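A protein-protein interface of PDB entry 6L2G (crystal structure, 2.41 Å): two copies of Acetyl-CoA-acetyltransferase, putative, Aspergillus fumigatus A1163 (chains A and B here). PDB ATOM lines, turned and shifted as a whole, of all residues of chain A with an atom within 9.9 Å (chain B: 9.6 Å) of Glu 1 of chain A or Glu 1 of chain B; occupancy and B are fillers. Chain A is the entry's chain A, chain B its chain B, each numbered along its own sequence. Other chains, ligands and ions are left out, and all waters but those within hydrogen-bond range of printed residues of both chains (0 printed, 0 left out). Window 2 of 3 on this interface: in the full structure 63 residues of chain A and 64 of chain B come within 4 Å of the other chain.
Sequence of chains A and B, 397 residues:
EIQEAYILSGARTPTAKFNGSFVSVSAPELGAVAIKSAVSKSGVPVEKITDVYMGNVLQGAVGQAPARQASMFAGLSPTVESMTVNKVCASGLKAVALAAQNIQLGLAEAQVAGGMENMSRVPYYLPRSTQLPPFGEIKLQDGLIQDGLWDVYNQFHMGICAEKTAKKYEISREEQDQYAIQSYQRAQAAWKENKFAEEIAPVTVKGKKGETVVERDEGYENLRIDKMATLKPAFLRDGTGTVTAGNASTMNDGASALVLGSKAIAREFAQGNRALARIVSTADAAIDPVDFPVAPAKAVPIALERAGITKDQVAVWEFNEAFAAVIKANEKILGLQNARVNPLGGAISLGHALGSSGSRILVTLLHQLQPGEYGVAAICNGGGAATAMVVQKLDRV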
ATOM      1  N   GLU A   1       1.461   5.826 -17.625  1.00  0.00           N
ATOM      2  CA  GLU A   1       2.585   4.980 -18.134  1.00  0.00           C
ATOM      3  C   GLU A   1       3.838   5.323 -17.311  1.00  0.00           C
ATOM      4  O   GLU A   1       4.774   5.932 -17.851  1.00  0.00           O
ATOM      5  CB  GLU A   1       2.720   5.136 -19.655  1.00  0.00           C
ATOM      6  CG  GLU A   1       3.029   6.551 -20.158  1.00  0.00           C
ATOM      7  CD  GLU A   1       2.064   7.670 -19.785  1.00  0.00           C
ATOM      8  OE1 GLU A   1       2.485   8.840 -19.846  1.00  0.00           O
ATOM      9  OE2 GLU A   1       0.898   7.376 -19.446  1.00  0.00           O
ATOM     10  N   ILE A   2       3.815   4.976 -16.019  1.00  0.00           N
ATOM     11  CA  ILE A   2       4.937   5.152 -15.046  1.00  0.00           C
ATOM     12  C   ILE A   2       6.129   4.312 -15.520  1.00  0.00           C
ATOM     13  O   ILE A   2       5.973   3.072 -15.560  1.00  0.00           O
ATOM     14  CB  ILE A   2       4.490   4.746 -13.626  1.00  0.00           C
ATOM     15  CG1 ILE A   2       3.495   5.758 -13.043  1.00  0.00           C
ATOM     16  CG2 ILE A   2       5.690   4.515 -12.708  1.00  0.00           C
ATOM     17  CD1 ILE A   2       2.989   5.402 -11.663  1.00  0.00           C
ATOM     18  N   GLN A   3       7.259   4.964 -15.835  1.00  0.00           N
ATOM     19  CA  GLN A   3       8.520   4.325 -16.305  1.00  0.00           C
ATOM     20  C   GLN A   3       9.301   3.770 -15.097  1.00  0.00           C
ATOM     21  O   GLN A   3       8.967   4.136 -13.953  1.00  0.00           O
ATOM     22  CB  GLN A   3       9.403   5.297 -17.106  1.00  0.00           C
ATOM     23  CG  GLN A   3       8.704   6.068 -18.231  1.00  0.00           C
ATOM     24  CD  GLN A   3       8.300   5.237 -19.431  1.00  0.00           C
ATOM     25  OE1 GLN A   3       8.986   4.298 -19.828  1.00  0.00           O
ATOM     26  NE2 GLN A   3       7.179   5.599 -20.039  1.00  0.00           N
ATOM     27  N   GLU A   4      10.283   2.902 -15.366  1.00  0.00           N
ATOM     28  CA  GLU A   4      11.220   2.300 -14.383  1.00  0.00           C
ATOM     29  C   GLU A   4      12.513   3.121 -14.367  1.00  0.00           C
ATOM     30  O   GLU A   4      12.857   3.696 -15.414  1.00  0.00           O
ATOM     31  CB  GLU A   4      11.537   0.857 -14.774  1.00  0.00           C
ATOM     32  CG  GLU A   4      10.350  -0.089 -14.683  1.00  0.00           C
ATOM     33  CD  GLU A   4      10.173  -0.755 -13.325  1.00  0.00           C
ATOM     34  OE1 GLU A   4       9.927  -1.987 -13.297  1.00  0.00           O
ATOM     35  OE2 GLU A   4      10.288  -0.045 -12.296  1.00  0.00           O
ATOM     36  N   GLN A 101      12.042   9.745  -9.619  1.00  0.00           N
ATOM     37  CA  GLN A 101      10.674  10.221  -9.985  1.00  0.00           C
ATOM     38  C   GLN A 101      10.700  10.958 -11.333  1.00  0.00           C
ATOM     39  O   GLN A 101       9.781  10.753 -12.141  1.00  0.00           O
ATOM     40  CB  GLN A 101      10.077  11.109  -8.890  1.00  0.00           C
ATOM     41  CG  GLN A 101       9.692  10.336  -7.636  1.00  0.00           C
ATOM     42  CD  GLN A 101       8.979  11.198  -6.617  1.00  0.00           C
ATOM     43  OE1 GLN A 101       8.609  12.339  -6.881  1.00  0.00           O
ATOM     44  NE2 GLN A 101       8.774  10.650  -5.433  1.00  0.00           N
ATOM     45  N   ASN A 102      11.720  11.766 -11.588  1.00  0.00           N
ATOM     46  CA  ASN A 102      11.885  12.467 -12.889  1.00  0.00           C
ATOM     47  C   ASN A 102      11.833  11.437 -14.024  1.00  0.00           C
ATOM     48  O   ASN A 102      11.127  11.676 -15.014  1.00  0.00           O
ATOM     49  CB  ASN A 102      13.144  13.338 -12.907  1.00  0.00           C
ATOM     50  CG  ASN A 102      12.942  14.641 -12.165  1.00  0.00           C
ATOM     51  OD1 ASN A 102      11.798  15.039 -11.910  1.00  0.00           O
ATOM     52  ND2 ASN A 102      14.036  15.311 -11.827  1.00  0.00           N
ATOM     53  N   ILE A 103      12.538  10.322 -13.862  1.00  0.00           N
ATOM     54  CA  ILE A 103      12.624   9.236 -14.873  1.00  0.00           C
ATOM     55  C   ILE A 103      11.285   8.490 -14.910  1.00  0.00           C
ATOM     56  O   ILE A 103      10.796   8.216 -16.035  1.00  0.00           O
ATOM     57  CB  ILE A 103      13.826   8.325 -14.582  1.00  0.00           C
ATOM     58  CG1 ILE A 103      15.129   9.082 -14.828  1.00  0.00           C
ATOM     59  CG2 ILE A 103      13.770   7.047 -15.414  1.00  0.00           C
ATOM     60  CD1 ILE A 103      16.316   8.465 -14.159  1.00  0.00           C
ATOM     61  N   GLN A 104      10.693   8.229 -13.743  1.00  0.00           N
ATOM     62  CA  GLN A 104       9.435   7.452 -13.611  1.00  0.00           C
ATOM     63  C   GLN A 104       8.310   8.196 -14.352  1.00  0.00           C
ATOM     64  O   GLN A 104       7.420   7.513 -14.895  1.00  0.00           O
ATOM     65  CB  GLN A 104       9.141   7.158 -12.134  1.00  0.00           C
ATOM     66  CG  GLN A 104      10.208   6.283 -11.470  1.00  0.00           C
ATOM     67  CD  GLN A 104      10.038   6.130  -9.974  1.00  0.00           C
ATOM     68  OE1 GLN A 104       9.144   6.695  -9.346  1.00  0.00           O
ATOM     69  NE2 GLN A 104      10.911   5.341  -9.374  1.00  0.00           N
ATOM     70  N   LEU A 105       8.353   9.532 -14.405  1.00  0.00           N
ATOM     71  CA  LEU A 105       7.273  10.373 -14.992  1.00  0.00           C
ATOM     72  C   LEU A 105       7.598  10.741 -16.445  1.00  0.00           C
ATOM     73  O   LEU A 105       6.775  11.450 -17.059  1.00  0.00           O
ATOM     74  CB  LEU A 105       7.089  11.634 -14.145  1.00  0.00           C
ATOM     75  CG  LEU A 105       6.578  11.418 -12.722  1.00  0.00           C
ATOM     76  CD1 LEU A 105       6.554  12.741 -11.967  1.00  0.00           C
ATOM     77  CD2 LEU A 105       5.204  10.793 -12.737  1.00  0.00           C
ATOM     78  N   GLY A 106       8.727  10.272 -16.986  1.00  0.00           N
ATOM     79  CA  GLY A 106       9.113  10.501 -18.392  1.00  0.00           C
ATOM     80  C   GLY A 106       9.646  11.905 -18.623  1.00  0.00           C
ATOM     81  O   GLY A 106       9.649  12.328 -19.778  1.00  0.00           O
ATOM     82  N   LEU A 107      10.108  12.600 -17.575  1.00  0.00           N
ATOM     83  CA  LEU A 107      10.573  14.013 -17.653  1.00  0.00           C
ATOM     84  C   LEU A 107      12.078  14.071 -17.917  1.00  0.00           C
ATOM     85  O   LEU A 107      12.560  15.149 -18.278  1.00  0.00           O
ATOM     86  CB  LEU A 107      10.235  14.736 -16.349  1.00  0.00           C
ATOM     87  CG  LEU A 107       8.766  14.704 -15.932  1.00  0.00           C
ATOM     88  CD1 LEU A 107       8.594  15.401 -14.595  1.00  0.00           C
ATOM     89  CD2 LEU A 107       7.886  15.353 -16.982  1.00  0.00           C
ATOM     90  N   GLU B   1      -1.280   5.319 -16.323  1.00  0.00           N
ATOM     91  CA  GLU B   1      -1.642   5.334 -14.876  1.00  0.00           C
ATOM     92  C   GLU B   1      -0.986   6.522 -14.150  1.00  0.00           C
ATOM     93  O   GLU B   1      -1.323   6.715 -12.963  1.00  0.00           O
ATOM     94  CB  GLU B   1      -1.341   3.985 -14.201  1.00  0.00           C
ATOM     95  CG  GLU B   1       0.102   3.490 -14.271  1.00  0.00           C
ATOM     96  CD  GLU B   1       0.299   2.260 -13.394  1.00  0.00           C
ATOM     97  OE1 GLU B   1      -0.095   2.305 -12.179  1.00  0.00           O
ATOM     98  OE2 GLU B   1       0.800   1.240 -13.929  1.00  0.00           O
ATOM     99  N   ILE B   2      -0.120   7.308 -14.802  1.00  0.00           N
ATOM    100  CA  ILE B   2       0.221   8.687 -14.323  1.00  0.00           C
ATOM    101  C   ILE B   2      -1.094   9.446 -14.081  1.00  0.00           C
ATOM    102  O   ILE B   2      -1.828   9.655 -15.049  1.00  0.00           O
ATOM    103  CB  ILE B   2       1.113   9.459 -15.318  1.00  0.00           C
ATOM    104  CG1 ILE B   2       2.523   8.874 -15.418  1.00  0.00           C
ATOM    105  CG2 ILE B   2       1.147  10.934 -14.938  1.00  0.00           C
ATOM    106  CD1 ILE B   2       3.424   9.605 -16.394  1.00  0.00           C
ATOM    107  N   GLN B   3      -1.377   9.834 -12.834  1.00  0.00           N
ATOM    108  CA  GLN B   3      -2.618  10.541 -12.438  1.00  0.00           C
ATOM    109  C   GLN B   3      -2.401  12.047 -12.568  1.00  0.00           C
ATOM    110  O   GLN B   3      -1.287  12.474 -12.928  1.00  0.00           O
ATOM    111  CB  GLN B   3      -2.989  10.204 -10.998  1.00  0.00           C
ATOM    112  CG  GLN B   3      -3.566   8.811 -10.804  1.00  0.00           C
ATOM    113  CD  GLN B   3      -3.710   8.530  -9.328  1.00  0.00           C
ATOM    114  OE1 GLN B   3      -4.407   9.247  -8.602  1.00  0.00           O
ATOM    115  NE2 GLN B   3      -3.008   7.505  -8.866  1.00  0.00           N
ATOM    116  N   GLU B   4      -3.427  12.822 -12.242  1.00  0.00           N
ATOM    117  CA  GLU B   4      -3.382  14.303 -12.263  1.00  0.00           C
ATOM    118  C   GLU B   4      -3.485  14.811 -10.823  1.00  0.00           C
ATOM    119  O   GLU B   4      -4.008  14.099  -9.952  1.00  0.00           O
ATOM    120  CB  GLU B   4      -4.460  14.862 -13.188  1.00  0.00           C
ATOM    121  CG  GLU B   4      -5.714  14.006 -13.271  1.00  0.00           C
ATOM    122  CD  GLU B   4      -6.660  14.408 -14.387  1.00  0.00           C
ATOM    123  OE1 GLU B   4      -7.838  13.969 -14.347  1.00  0.00           O
ATOM    124  OE2 GLU B   4      -6.210  15.153 -15.299  1.00  0.00           O
ATOM    125  N   GLN B 101       4.030  15.460  -7.669  1.00  0.00           N
ATOM    126  CA  GLN B 101       4.626  14.230  -8.241  1.00  0.00           C
ATOM    127  C   GLN B 101       4.165  13.031  -7.416  1.00  0.00           C
ATOM    128  O   GLN B 101       3.858  12.002  -8.006  1.00  0.00           O
ATOM    129  CB  GLN B 101       6.144  14.346  -8.315  1.00  0.00           C
ATOM    130  CG  GLN B 101       6.594  15.229  -9.465  1.00  0.00           C
ATOM    131  CD  GLN B 101       8.091  15.261  -9.632  1.00  0.00           C
ATOM    132  OE1 GLN B 101       8.833  14.484  -9.015  1.00  0.00           O
ATOM    133  NE2 GLN B 101       8.532  16.192 -10.460  1.00  0.00           N
ATOM    134  N   ASN B 102       4.086  13.189  -6.101  1.00  0.00           N
ATOM    135  CA  ASN B 102       3.615  12.135  -5.171  1.00  0.00           C
ATOM    136  C   ASN B 102       2.205  11.693  -5.573  1.00  0.00           C
ATOM    137  O   ASN B 102       1.978  10.477  -5.625  1.00  0.00           O
ATOM    138  CB  ASN B 102       3.736  12.617  -3.734  1.00  0.00           C
ATOM    139  CG  ASN B 102       5.160  12.504  -3.232  1.00  0.00           C
ATOM    140  OD1 ASN B 102       5.991  11.850  -3.867  1.00  0.00           O
ATOM    141  ND2 ASN B 102       5.430  13.078  -2.068  1.00  0.00           N
ATOM    142  N   ILE B 103       1.324  12.637  -5.910  1.00  0.00           N
ATOM    143  CA  ILE B 103      -0.057  12.363  -6.403  1.00  0.00           C
ATOM    144  C   ILE B 103       0.003  11.774  -7.830  1.00  0.00           C
ATOM    145  O   ILE B 103      -0.593  10.698  -8.080  1.00  0.00           O
ATOM    146  CB  ILE B 103      -0.889  13.657  -6.324  1.00  0.00           C
ATOM    147  CG1 ILE B 103      -1.021  14.122  -4.871  1.00  0.00           C
ATOM    148  CG2 ILE B 103      -2.242  13.496  -7.017  1.00  0.00           C
ATOM    149  CD1 ILE B 103      -1.595  15.523  -4.696  1.00  0.00           C
ATOM    150  N   GLN B 104       0.741  12.405  -8.733  1.00  0.00           N
ATOM    151  CA  GLN B 104       0.865  11.939 -10.136  1.00  0.00           C
ATOM    152  C   GLN B 104       1.341  10.473 -10.155  1.00  0.00           C
ATOM    153  O   GLN B 104       1.067   9.772 -11.131  1.00  0.00           O
ATOM    154  CB  GLN B 104       1.799  12.879 -10.915  1.00  0.00           C
ATOM    155  CG  GLN B 104       1.204  14.276 -11.140  1.00  0.00           C
ATOM    156  CD  GLN B 104       2.177  15.314 -11.656  1.00  0.00           C
ATOM    157  OE1 GLN B 104       3.367  15.064 -11.825  1.00  0.00           O
ATOM    158  NE2 GLN B 104       1.671  16.512 -11.909  1.00  0.00           N
ATOM    159  N   LEU B 105       2.061  10.018  -9.134  1.00  0.00           N
ATOM    160  CA  LEU B 105       2.717   8.688  -9.157  1.00  0.00           C
ATOM    161  C   LEU B 105       1.889   7.670  -8.374  1.00  0.00           C
ATOM    162  O   LEU B 105       2.331   6.521  -8.314  1.00  0.00           O
ATOM    163  CB  LEU B 105       4.121   8.800  -8.559  1.00  0.00           C
ATOM    164  CG  LEU B 105       5.225   9.273  -9.500  1.00  0.00           C
ATOM    165  CD1 LEU B 105       6.506   9.494  -8.717  1.00  0.00           C
ATOM    166  CD2 LEU B 105       5.461   8.268 -10.623  1.00  0.00           C
ATOM    167  N   GLY B 106       0.764   8.082  -7.782  1.00  0.00           N
ATOM    168  CA  GLY B 106      -0.127   7.182  -7.030  1.00  0.00           C
ATOM    169  C   GLY B 106       0.320   6.984  -5.597  1.00  0.00           C
ATOM    170  O   GLY B 106      -0.376   6.274  -4.874  1.00  0.00           O
ATOM    171  N   LEU B 107       1.399   7.638  -5.169  1.00  0.00           N
ATOM    172  CA  LEU B 107       2.027   7.415  -3.835  1.00  0.00           C
ATOM    173  C   LEU B 107       1.260   8.158  -2.738  1.00  0.00           C
ATOM    174  O   LEU B 107       1.492   7.860  -1.568  1.00  0.00           O
ATOM    175  CB  LEU B 107       3.480   7.893  -3.875  1.00  0.00           C
ATOM    176  CG  LEU B 107       4.348   7.269  -4.965  1.00  0.00           C
ATOM    177  CD1 LEU B 107       5.731   7.912  -4.986  1.00  0.00           C
ATOM    178  CD2 LEU B 107       4.446   5.762  -4.779  1.00  0.00           C
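N of Glu 1 of chain A lies close to N of Glu 1 of chain B, at 3.1 Å.
The side-chain amide oxygen (OE1) of Gln 101 of chain B lies close to the side-chain amide oxygen (OE1) of Gln 101 of chain A (3.0 Å).
NE2 of Gln 101 of chain A sits at hydrogen-bond distance from OD1 of Asn 102 of chain B, at 3.4 Å.
The backbone carbonyl oxygen (O) of Asn 102 of chain A sits at hydrogen-bond distance from the backbone NH (N) of Leu 107 of chain A, 2.9 Å away.
The backbone carbonyl oxygen of Asn 102 of chain B lies within hydrogen-bond range of the backbone NH of Leu 107 of chain B, 2.9 Å away.
NE2 of Gln 3 of chain A sits at hydrogen-bond distance from O of Glu 1 of chain A, at 3.3 Å.
The backbone NH (N) of Gln 3 of chain B is in hydrogen-bond range of the backbone carbonyl oxygen (O) of Gln 104 of chain B, at 3.0 Å.
N of Gln 3 of chain A sits at hydrogen-bond distance from O of Gln 104 of chain A, at 2.7 Å.
Among the printed residues, pairs that only touch across the chains: Leu 105 of chain A with Leu 105 of chain B (3.3 Å), Gln 101 of chain A with Leu 105 of chain B (3.5 Å), Leu 105 of chain A with Gln 101 of chain B (3.5 Å), Glu 1 of chain A with Ile 2 of chain B (3.6 Å), Ile 2 of chain A with Leu 105 of chain B (3.6 Å), Asn 102 of chain A with Gln 101 of chain B (3.8 Å), Leu 105 of chain A with Ile 2 of chain B (3.9 Å), Gln 104 of chain A with Leu 105 of chain B (3.9 Å) and Leu 105 of chain A with Gln 104 of chain B (3.9 Å).
Of the printed residues of chain B, Leu 105 of chain A touches Ile 2, Gln 101, Gln 104 and Leu 105.
Glu 1 of chain B touches one residue of chain A.
Glu 4 of chain B touches none of the printed residues of chain A.
Printed residues of chain A within 4 Å of Gln 101 of chain B: Gln 101 (3.0 Å), Asn 102 (3.8 Å) and Leu 105 (3.5 Å).
Of the printed residues of chain A, Leu 105 of chain B touches Ile 2, Gln 101, Gln 104 and Leu 105.
Gly 106 of chain B touches none of the printed residues of chain A.
The nearest residue of chain A that does not touch Glu 1 of chain B is Ile 2 of chain A (4.3 Å).
Hydrophobic or aromatic side chains of chain B that line the printed part of chain A: Ile 2 and Leu 105.
Among the printed residues, 12 pairs touch across the chains.
Among the printed residues, no Asp or Glu carboxylate lies within 4 Å of a Lys or Arg side-chain nitrogen of the other chain.
Gln 101 of chain B touches its own counterpart, Gln 101 of chain A.
Gln 101 of chain A touches Asn 102 of chain B, and with the chains exchanged Asn 102 of chain A touches Gln 101 of chain B.
Gln 104 of chain A touches Leu 105 of chain B, and with the chains exchanged Leu 105 of chain A touches Gln 104 of chain B.
Leu 105 of chain B touches its own counterpart, Leu 105 of chain A.
11 positions are printed for both chains.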
